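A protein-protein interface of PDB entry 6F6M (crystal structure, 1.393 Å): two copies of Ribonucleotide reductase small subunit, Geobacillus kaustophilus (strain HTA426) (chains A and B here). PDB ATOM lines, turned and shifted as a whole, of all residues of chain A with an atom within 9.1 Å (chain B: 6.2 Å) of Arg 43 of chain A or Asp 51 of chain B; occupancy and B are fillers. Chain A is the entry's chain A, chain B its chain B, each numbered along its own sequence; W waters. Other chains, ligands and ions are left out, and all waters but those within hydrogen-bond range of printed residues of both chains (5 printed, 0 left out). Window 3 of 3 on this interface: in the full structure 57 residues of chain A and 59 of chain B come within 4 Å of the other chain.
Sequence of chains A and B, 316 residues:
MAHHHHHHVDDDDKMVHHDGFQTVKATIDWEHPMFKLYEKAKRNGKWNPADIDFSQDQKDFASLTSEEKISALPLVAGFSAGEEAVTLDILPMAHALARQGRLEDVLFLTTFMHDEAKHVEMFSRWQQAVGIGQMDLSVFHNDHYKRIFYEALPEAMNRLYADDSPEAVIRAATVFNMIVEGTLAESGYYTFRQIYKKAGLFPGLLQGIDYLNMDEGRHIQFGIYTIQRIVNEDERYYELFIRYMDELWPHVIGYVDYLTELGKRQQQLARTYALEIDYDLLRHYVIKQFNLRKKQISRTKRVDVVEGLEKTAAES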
ATOM      1  N   LYS A  36      10.600   9.558  23.260  1.00  0.00           N
ATOM      2  CA  LYS A  36      10.456  10.250  24.538  1.00  0.00           C
ATOM      3  C   LYS A  36      11.804  10.763  25.023  1.00  0.00           C
ATOM      4  O   LYS A  36      11.902  11.879  25.554  1.00  0.00           O
ATOM      5  CB  LYS A  36       9.802   9.330  25.568  1.00  0.00           C
ATOM      6  CG  LYS A  36       8.401   8.907  25.145  1.00  0.00           C
ATOM      7  CD  LYS A  36       7.369   8.984  26.245  1.00  0.00           C
ATOM      8  CE  LYS A  36       6.009   9.448  25.704  1.00  0.00           C
ATOM      9  NZ  LYS A  36       5.357  10.435  26.620  1.00  0.00           N
ATOM     10  N   LEU A  37      12.882   9.997  24.772  1.00  0.00           N
ATOM     11  CA  LEU A  37      14.212  10.475  25.161  1.00  0.00           C
ATOM     12  C   LEU A  37      14.651  11.662  24.297  1.00  0.00           C
ATOM     13  O   LEU A  37      15.295  12.592  24.776  1.00  0.00           O
ATOM     14  CB  LEU A  37      15.215   9.334  25.051  1.00  0.00           C
ATOM     15  CG  LEU A  37      16.555   9.519  25.737  1.00  0.00           C
ATOM     16  CD1 LEU A  37      16.412   9.730  27.256  1.00  0.00           C
ATOM     17  CD2 LEU A  37      17.444   8.307  25.442  1.00  0.00           C
ATOM     18  N   TYR A  38      14.315  11.631  23.016  1.00  0.00           N
ATOM     19  CA  TYR A  38      14.544  12.756  22.112  1.00  0.00           C
ATOM     20  C   TYR A  38      13.848  14.015  22.612  1.00  0.00           C
ATOM     21  O   TYR A  38      14.444  15.092  22.648  1.00  0.00           O
ATOM     22  CB  TYR A  38      14.013  12.342  20.730  1.00  0.00           C
ATOM     23  CG  TYR A  38      13.804  13.435  19.714  1.00  0.00           C
ATOM     24  CD1 TYR A  38      14.880  14.054  19.115  1.00  0.00           C
ATOM     25  CD2 TYR A  38      12.540  13.817  19.305  1.00  0.00           C
ATOM     26  CE1 TYR A  38      14.697  15.031  18.165  1.00  0.00           C
ATOM     27  CE2 TYR A  38      12.346  14.801  18.326  1.00  0.00           C
ATOM     28  CZ  TYR A  38      13.432  15.411  17.772  1.00  0.00           C
ATOM     29  OH  TYR A  38      13.287  16.396  16.800  1.00  0.00           O
ATOM     30  N   GLU A  39      12.597  13.885  23.049  1.00  0.00           N
ATOM     31  CA  GLU A  39      11.863  15.034  23.568  1.00  0.00           C
ATOM     32  C   GLU A  39      12.542  15.604  24.807  1.00  0.00           C
ATOM     33  O   GLU A  39      12.654  16.826  24.958  1.00  0.00           O
ATOM     34  CB  GLU A  39      10.426  14.612  23.875  1.00  0.00           C
ATOM     35  CG  GLU A  39       9.591  14.400  22.634  1.00  0.00           C
ATOM     36  CD  GLU A  39       9.276  15.726  21.976  1.00  0.00           C
ATOM     37  OE1 GLU A  39       8.933  16.675  22.687  1.00  0.00           O
ATOM     38  OE2 GLU A  39       9.426  15.840  20.763  1.00  0.00           O
ATOM     39  N   LYS A  40      13.018  14.725  25.694  1.00  0.00           N
ATOM     40  CA  LYS A  40      13.720  15.170  26.893  1.00  0.00           C
ATOM     41  C   LYS A  40      15.024  15.864  26.526  1.00  0.00           C
ATOM     42  O   LYS A  40      15.388  16.882  27.127  1.00  0.00           O
ATOM     43  CB  LYS A  40      13.971  13.954  27.794  1.00  0.00           C
ATOM     44  CG  LYS A  40      14.642  14.229  29.130  1.00  0.00           C
ATOM     45  CD  LYS A  40      14.837  12.928  29.901  1.00  0.00           C
ATOM     46  CE  LYS A  40      15.367  13.153  31.310  1.00  0.00           C
ATOM     47  NZ  LYS A  40      15.614  11.862  32.025  1.00  0.00           N
ATOM     48  N   ALA A  41      15.741  15.318  25.535  1.00  0.00           N
ATOM     49  CA  ALA A  41      17.006  15.908  25.110  1.00  0.00           C
ATOM     50  C   ALA A  41      16.824  17.325  24.591  1.00  0.00           C
ATOM     51  O   ALA A  41      17.649  18.201  24.871  1.00  0.00           O
ATOM     52  CB  ALA A  41      17.638  15.058  24.006  1.00  0.00           C
ATOM     53  N   LYS A  42      15.748  17.588  23.838  1.00  0.00           N
ATOM     54  CA  LYS A  42      15.519  18.955  23.363  1.00  0.00           C
ATOM     55  C   LYS A  42      15.210  19.896  24.524  1.00  0.00           C
ATOM     56  O   LYS A  42      15.652  21.060  24.536  1.00  0.00           O
ATOM     57  CB  LYS A  42      14.344  19.002  22.400  1.00  0.00           C
ATOM     58  CG  LYS A  42      14.615  18.364  21.045  1.00  0.00           C
ATOM     59  CD  LYS A  42      13.424  18.438  20.131  1.00  0.00           C
ATOM     60  CE  LYS A  42      12.356  17.510  20.577  1.00  0.00           C
ATOM     61  NZ  LYS A  42      11.070  17.863  19.968  1.00  0.00           N
ATOM     62  N   ARG A  43      14.433  19.425  25.504  1.00  0.00           N
ATOM     63  CA  ARG A  43      14.059  20.320  26.591  1.00  0.00           C
ATOM     64  C   ARG A  43      15.193  20.554  27.566  1.00  0.00           C
ATOM     65  O   ARG A  43      15.218  21.618  28.187  1.00  0.00           O
ATOM     66  CB  ARG A  43      12.857  19.789  27.360  1.00  0.00           C
ATOM     67  CG  ARG A  43      11.615  19.723  26.500  1.00  0.00           C
ATOM     68  CD  ARG A  43      10.383  20.010  27.277  1.00  0.00           C
ATOM     69  NE  ARG A  43       9.179  19.820  26.471  1.00  0.00           N
ATOM     70  CZ  ARG A  43       8.582  20.768  25.749  1.00  0.00           C
ATOM     71  NH1 ARG A  43       9.067  22.000  25.701  1.00  0.00           N
ATOM     72  NH2 ARG A  43       7.484  20.477  25.065  1.00  0.00           N
ATOM     73  N   ASN A  44      16.134  19.594  27.710  1.00  0.00           N
ATOM     74  CA  ASN A  44      17.171  19.672  28.722  1.00  0.00           C
ATOM     75  C   ASN A  44      18.549  19.989  28.148  1.00  0.00           C
ATOM     76  O   ASN A  44      19.447  20.348  28.909  1.00  0.00           O
ATOM     77  CB  ASN A  44      17.209  18.354  29.542  1.00  0.00           C
ATOM     78  CG  ASN A  44      15.806  17.936  30.144  1.00  0.00           C
ATOM     79  OD1 ASN A  44      14.836  18.712  30.160  1.00  0.00           O
ATOM     80  ND2 ASN A  44      15.732  16.706  30.669  1.00  0.00           N
ATOM     81  N   GLY A  45      18.732  19.871  26.842  1.00  0.00           N
ATOM     82  CA  GLY A  45      20.053  20.017  26.239  1.00  0.00           C
ATOM     83  C   GLY A  45      20.253  21.329  25.513  1.00  0.00           C
ATOM     84  O   GLY A  45      20.632  21.341  24.344  1.00  0.00           O
ATOM     85  N   LYS A  46      20.055  22.448  26.213  1.00  0.00           N
ATOM     86  CA  LYS A  46      20.081  23.771  25.598  1.00  0.00           C
ATOM     87  C   LYS A  46      21.403  24.518  25.799  1.00  0.00           C
ATOM     88  O   LYS A  46      21.622  25.546  25.142  1.00  0.00           O
ATOM     89  CB  LYS A  46      18.931  24.635  26.144  1.00  0.00           C
ATOM     90  CG  LYS A  46      17.499  24.098  25.888  1.00  0.00           C
ATOM     91  CD  LYS A  46      17.009  24.385  24.476  1.00  0.00           C
ATOM     92  CE  LYS A  46      15.513  24.033  24.305  1.00  0.00           C
ATOM     93  NZ  LYS A  46      15.196  23.299  23.018  1.00  0.00           N
ATOM     94  N   TRP A  47      22.288  24.039  26.670  1.00  0.00           N
ATOM     95  CA  TRP A  47      23.485  24.801  26.993  1.00  0.00           C
ATOM     96  C   TRP A  47      24.390  24.982  25.787  1.00  0.00           C
ATOM     97  O   TRP A  47      24.415  24.172  24.866  1.00  0.00           O
ATOM     98  CB  TRP A  47      24.276  24.127  28.114  1.00  0.00           C
ATOM     99  CG  TRP A  47      24.953  22.838  27.789  1.00  0.00           C
ATOM    100  CD1 TRP A  47      24.370  21.633  27.543  1.00  0.00           C
ATOM    101  CD2 TRP A  47      26.364  22.619  27.733  1.00  0.00           C
ATOM    102  NE1 TRP A  47      25.336  20.668  27.325  1.00  0.00           N
ATOM    103  CE2 TRP A  47      26.568  21.257  27.414  1.00  0.00           C
ATOM    104  CE3 TRP A  47      27.472  23.442  27.903  1.00  0.00           C
ATOM    105  CZ2 TRP A  47      27.831  20.703  27.336  1.00  0.00           C
ATOM    106  CZ3 TRP A  47      28.723  22.892  27.794  1.00  0.00           C
ATOM    107  CH2 TRP A  47      28.896  21.537  27.496  1.00  0.00           C
ATOM    108  N   THR A 111      20.400  14.232  18.684  1.00  0.00           N
ATOM    109  CA  THR A 111      20.711  14.975  19.908  1.00  0.00           C
ATOM    110  C   THR A 111      21.954  14.409  20.581  1.00  0.00           C
ATOM    111  O   THR A 111      22.768  15.165  21.118  1.00  0.00           O
ATOM    112  CB  THR A 111      19.524  15.012  20.885  1.00  0.00           C
ATOM    113  OG1 THR A 111      19.350  13.771  21.582  1.00  0.00           O
ATOM    114  CG2 THR A 111      18.218  15.401  20.186  1.00  0.00           C
ATOM    115  N   MET A 214      24.816  15.822  32.631  1.00  0.00           N
ATOM    116  CA  MET A 214      23.376  15.735  32.385  1.00  0.00           C
ATOM    117  C   MET A 214      23.087  15.135  31.010  1.00  0.00           C
ATOM    118  O   MET A 214      22.229  14.251  30.879  1.00  0.00           O
ATOM    119  CB  MET A 214      22.691  17.104  32.496  1.00  0.00           C
ATOM    120  CG  MET A 214      22.657  17.746  33.837  1.00  0.00           C
ATOM    121  SD  MET A 214      21.338  18.994  33.894  1.00  0.00           S
ATOM    122  CE  MET A 214      21.910  20.301  32.803  1.00  0.00           C
ATOM    123  N   ASP A 215      23.784  15.617  29.970  1.00  0.00           N
ATOM    124  CA  ASP A 215      23.605  15.049  28.640  1.00  0.00           C
ATOM    125  C   ASP A 215      23.905  13.563  28.664  1.00  0.00           C
ATOM    126  O   ASP A 215      23.161  12.753  28.099  1.00  0.00           O
ATOM    127  CB  ASP A 215      24.595  15.691  27.682  1.00  0.00           C
ATOM    128  CG  ASP A 215      24.357  17.154  27.418  1.00  0.00           C
ATOM    129  OD1 ASP A 215      23.228  17.652  27.584  1.00  0.00           O
ATOM    130  OD2 ASP A 215      25.342  17.810  26.977  1.00  0.00           O
ATOM    131  N   ARG A 218      21.400  10.747  29.317  1.00  0.00           N
ATOM    132  CA  ARG A 218      20.541  10.288  28.234  1.00  0.00           C
ATOM    133  C   ARG A 218      21.269   9.290  27.367  1.00  0.00           C
ATOM    134  O   ARG A 218      20.677   8.313  26.894  1.00  0.00           O
ATOM    135  CB  ARG A 218      20.098  11.449  27.362  1.00  0.00           C
ATOM    136  CG  ARG A 218      19.235  12.430  28.107  1.00  0.00           C
ATOM    137  CD  ARG A 218      18.631  13.446  27.140  1.00  0.00           C
ATOM    138  NE  ARG A 218      19.654  14.296  26.529  1.00  0.00           N
ATOM    139  CZ  ARG A 218      20.177  15.395  27.078  1.00  0.00           C
ATOM    140  NH1 ARG A 218      19.812  15.791  28.291  1.00  0.00           N
ATOM    141  NH2 ARG A 218      21.094  16.095  26.431  1.00  0.00           N
ATOM    142  N   TRP B  47      14.470  26.557  18.317  1.00  0.00           N
ATOM    143  CA  TRP B  47      13.055  26.217  18.332  1.00  0.00           C
ATOM    144  C   TRP B  47      12.834  24.725  18.574  1.00  0.00           C
ATOM    145  O   TRP B  47      13.666  23.874  18.247  1.00  0.00           O
ATOM    146  CB  TRP B  47      12.392  26.617  17.012  1.00  0.00           C
ATOM    147  CG  TRP B  47      12.745  25.820  15.794  1.00  0.00           C
ATOM    148  CD1 TRP B  47      13.934  25.801  15.141  1.00  0.00           C
ATOM    149  CD2 TRP B  47      11.858  24.977  15.054  1.00  0.00           C
ATOM    150  NE1 TRP B  47      13.851  24.977  14.030  1.00  0.00           N
ATOM    151  CE2 TRP B  47      12.581  24.468  13.962  1.00  0.00           C
ATOM    152  CE3 TRP B  47      10.518  24.605  15.202  1.00  0.00           C
ATOM    153  CZ2 TRP B  47      12.005  23.608  13.033  1.00  0.00           C
ATOM    154  CZ3 TRP B  47       9.954  23.757  14.281  1.00  0.00           C
ATOM    155  CH2 TRP B  47      10.696  23.263  13.210  1.00  0.00           C
ATOM    156  N   ASN B  48      11.644  24.415  19.078  1.00  0.00           N
ATOM    157  CA  ASN B  48      11.233  23.056  19.386  1.00  0.00           C
ATOM    158  C   ASN B  48       9.863  22.840  18.760  1.00  0.00           C
ATOM    159  O   ASN B  48       8.901  23.557  19.122  1.00  0.00           O
ATOM    160  CB  ASN B  48      11.184  22.840  20.898  1.00  0.00           C
ATOM    161  CG  ASN B  48      10.897  21.411  21.256  1.00  0.00           C
ATOM    162  OD1 ASN B  48      10.457  20.631  20.411  1.00  0.00           O
ATOM    163  ND2 ASN B  48      11.074  21.066  22.522  1.00  0.00           N
ATOM    164  N   PRO B  49       9.718  21.901  17.809  1.00  0.00           N
ATOM    165  CA  PRO B  49       8.395  21.670  17.201  1.00  0.00           C
ATOM    166  C   PRO B  49       7.319  21.336  18.201  1.00  0.00           C
ATOM    167  O   PRO B  49       6.139  21.594  17.933  1.00  0.00           O
ATOM    168  CB  PRO B  49       8.638  20.475  16.271  1.00  0.00           C
ATOM    169  CG  PRO B  49      10.110  20.548  15.942  1.00  0.00           C
ATOM    170  CD  PRO B  49      10.774  21.106  17.174  1.00  0.00           C
ATOM    171  N   ALA B  50       7.699  20.740  19.330  1.00  0.00           N
ATOM    172  CA  ALA B  50       6.743  20.361  20.356  1.00  0.00           C
ATOM    173  C   ALA B  50       6.087  21.572  21.001  1.00  0.00           C
ATOM    174  O   ALA B  50       5.067  21.421  21.688  1.00  0.00           O
ATOM    175  CB  ALA B  50       7.474  19.525  21.401  1.00  0.00           C
ATOM    176  N   ASP B  51       6.663  22.750  20.833  1.00  0.00           N
ATOM    177  CA  ASP B  51       6.136  23.976  21.430  1.00  0.00           C
ATOM    178  C   ASP B  51       5.183  24.733  20.505  1.00  0.00           C
ATOM    179  O   ASP B  51       4.582  25.730  20.921  1.00  0.00           O
ATOM    180  CB  ASP B  51       7.291  24.877  21.851  1.00  0.00           C
ATOM    181  CG  ASP B  51       8.066  24.304  23.017  1.00  0.00           C
ATOM    182  OD1 ASP B  51       7.482  23.489  23.777  1.00  0.00           O
ATOM    183  OD2 ASP B  51       9.263  24.644  23.155  1.00  0.00           O
ATOM    184  N   ILE B  52       4.995  24.276  19.282  1.00  0.00           N
ATOM    185  CA  ILE B  52       4.101  24.952  18.354  1.00  0.00           C
ATOM    186  C   ILE B  52       2.670  24.568  18.682  1.00  0.00           C
ATOM    187  O   ILE B  52       2.351  23.386  18.878  1.00  0.00           O
ATOM    188  CB  ILE B  52       4.445  24.584  16.903  1.00  0.00           C
ATOM    189  CG1 ILE B  52       5.836  25.122  16.564  1.00  0.00           C
ATOM    190  CG2 ILE B  52       3.376  25.135  15.948  1.00  0.00           C
ATOM    191  CD1 ILE B  52       6.305  24.768  15.195  1.00  0.00           C
ATOM    192  N   ASP B  53       1.808  25.572  18.739  1.00  0.00           N
ATOM    193  CA  ASP B  53       0.374  25.377  18.930  1.00  0.00           C
ATOM    194  C   ASP B  53      -0.268  25.095  17.570  1.00  0.00           C
ATOM    195  O   ASP B  53      -0.351  25.987  16.717  1.00  0.00           O
ATOM    196  CB  ASP B  53      -0.208  26.636  19.569  1.00  0.00           C
ATOM    197  CG  ASP B  53      -1.676  26.512  19.904  1.00  0.00           C
ATOM    198  OD1 ASP B  53      -2.280  25.461  19.620  1.00  0.00           O
ATOM    199  OD2 ASP B  53      -2.236  27.505  20.449  1.00  0.00           O
ATOM    200  N   ARG B 125       3.935  16.133  13.332  1.00  0.00           N
ATOM    201  CA  ARG B 125       3.037  16.672  14.353  1.00  0.00           C
ATOM    202  C   ARG B 125       1.852  17.369  13.717  1.00  0.00           C
ATOM    203  O   ARG B 125       0.723  17.273  14.219  1.00  0.00           O
ATOM    204  CB  ARG B 125       3.770  17.662  15.250  1.00  0.00           C
ATOM    205  CG  ARG B 125       4.694  17.037  16.260  1.00  0.00           C
ATOM    206  CD  ARG B 125       5.289  18.071  17.170  1.00  0.00           C
ATOM    207  NE  ARG B 125       6.131  17.461  18.197  1.00  0.00           N
ATOM    208  CZ  ARG B 125       5.690  16.919  19.323  1.00  0.00           C
ATOM    209  NH1 ARG B 125       4.388  16.926  19.626  1.00  0.00           N
ATOM    210  NH2 ARG B 125       6.568  16.371  20.156  1.00  0.00           N
ATOM    211  N   GLN B 207       4.258  28.919  11.231  1.00  0.00           N
ATOM    212  CA  GLN B 207       5.326  29.146  12.206  1.00  0.00           C
ATOM    213  C   GLN B 207       6.444  28.120  12.039  1.00  0.00           C
ATOM    214  O   GLN B 207       7.636  28.467  12.036  1.00  0.00           O
ATOM    215  CB  GLN B 207       4.742  29.064  13.617  1.00  0.00           C
ATOM    216  CG  GLN B 207       5.698  29.519  14.705  1.00  0.00           C
ATOM    217  CD  GLN B 207       5.044  29.602  16.079  1.00  0.00           C
ATOM    218  OE1 GLN B 207       4.045  28.943  16.335  1.00  0.00           O
ATOM    219  NE2 GLN B 207       5.605  30.432  16.961  1.00  0.00           N
HETATM  220  O   HOH W   1      10.701  18.353  23.566  1.00  0.00           O
HETATM  221  O   HOH W   2       4.827  21.854  24.478  1.00  0.00           O
HETATM  222  O   HOH W   3      14.556  22.180  20.429  1.00  0.00           O
HETATM  223  O   HOH W   4      11.647  23.450  24.316  1.00  0.00           O
HETATM  224  O   HOH W   5       6.213  23.639  26.715  1.00  0.00           O
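The side-chain amino group (NZ) of Lys 42 of chain A sits at hydrogen-bond distance from the side-chain amide oxygen (OD1) of Asn 48 of chain B. The side-chain carboxylate (OD1) of Asp 51 of chain B lies within salt-bridge range of the guanidinium group (NH1) of Arg 43 of chain A (2.9 Å). The guanidinium group (NH2) of Arg 125 of chain B lies within salt-bridge range of the side-chain carboxylate (OE2) of Glu 39 of chain A (3.0 Å).
Of chain A, only Arg 43 (2.9 Å) comes within 4 Å of Asp 51 of chain B. Asn 48 of chain B touches just these residues of chain A: Lys 42 and Arg 43. Printed residues of chain A within 4 Å of Ala 50 of chain B: Glu 39 (3.5 Å) and Arg 43 (3.8 Å). Of the printed residues of chain A, Arg 125 of chain B touches Glu 39. Printed residues of chain B within 4 Å of Glu 39 of chain A: Ala 50 (3.5 Å) and Arg 125 (3.0 Å). Of the printed residues of chain B, Lys 42 of chain A touches Asn 48 (2.9 Å). The nearest printed residue of chain B that does not touch Arg 43 of chain A is Arg 125 of chain B (6.5 Å). The nearest residue of chain A that does not touch Asp 51 of chain B is Lys 46 of chain A (6.1 Å).
Of the 16 printed residues of chain A, 3 touch a printed residue of chain B. Printed residues of chain A that touch a printed residue of chain B: Glu 39, Lys 42 and Arg 43. Of the 9 printed residues of chain B, 4 touch a printed residue of chain A. Hydrophobic or aromatic side chains of chain B that line the printed part of chain A: Ala 50.
NZ of Lys 46 of chain A is in hydrogen-bond range of O of Lys 42 of chain A (2.7 Å). OD1 of Asn 48 of chain B sits at hydrogen-bond distance from N of Ala 50 of chain B (3.0 Å). OE2 of Glu 39 of chain A lies within salt-bridge range of NZ of Lys 42 of chain A, 2.7 Å away.
Water W1 lies within hydrogen-bond range of OE1 of Glu 39 of chain A (2.6 Å) and ND2 of Asn 48 of chain B (2.9 Å). Water W2 lies within hydrogen-bond range of O of Ala 50 of chain B (2.8 Å), NH2 of Arg 43 of chain A (3.0 Å) and OD1 of Asp 51 of chain B (3.2 Å). Water W3 lies within hydrogen-bond range of NZ of Lys 46 of chain A (2.9 Å) and O of Trp 47 of chain B (2.9 Å). Water W4 lies within hydrogen-bond range of the side-chain carboxylate (OD2) of Asp 51 of chain B (2.9 Å), the side-chain amide nitrogen (ND2) of Asn 48 of chain B (3.0 Å) and the guanidinium group (NH1) of Arg 43 of chain A (3.3 Å). Water W5 bridges OD1 of Asp 51 of chain B (3.2 Å) and NH1 of Arg 43 of chain A (3.4 Å).
1 position is printed for both chains. Of the 6 pairs that touch across the chains among the printed residues, none has its exchanged pair printed and touching as well.
Among the printed residues, merely in contact across the chains: Glu 39 of chain A with Ala 50 of chain B (3.5 Å), Arg 43 of chain A with Ala 50 of chain B (3.8 Å) and Arg 43 of chain A with Asn 48 of chain B (3.9 Å).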
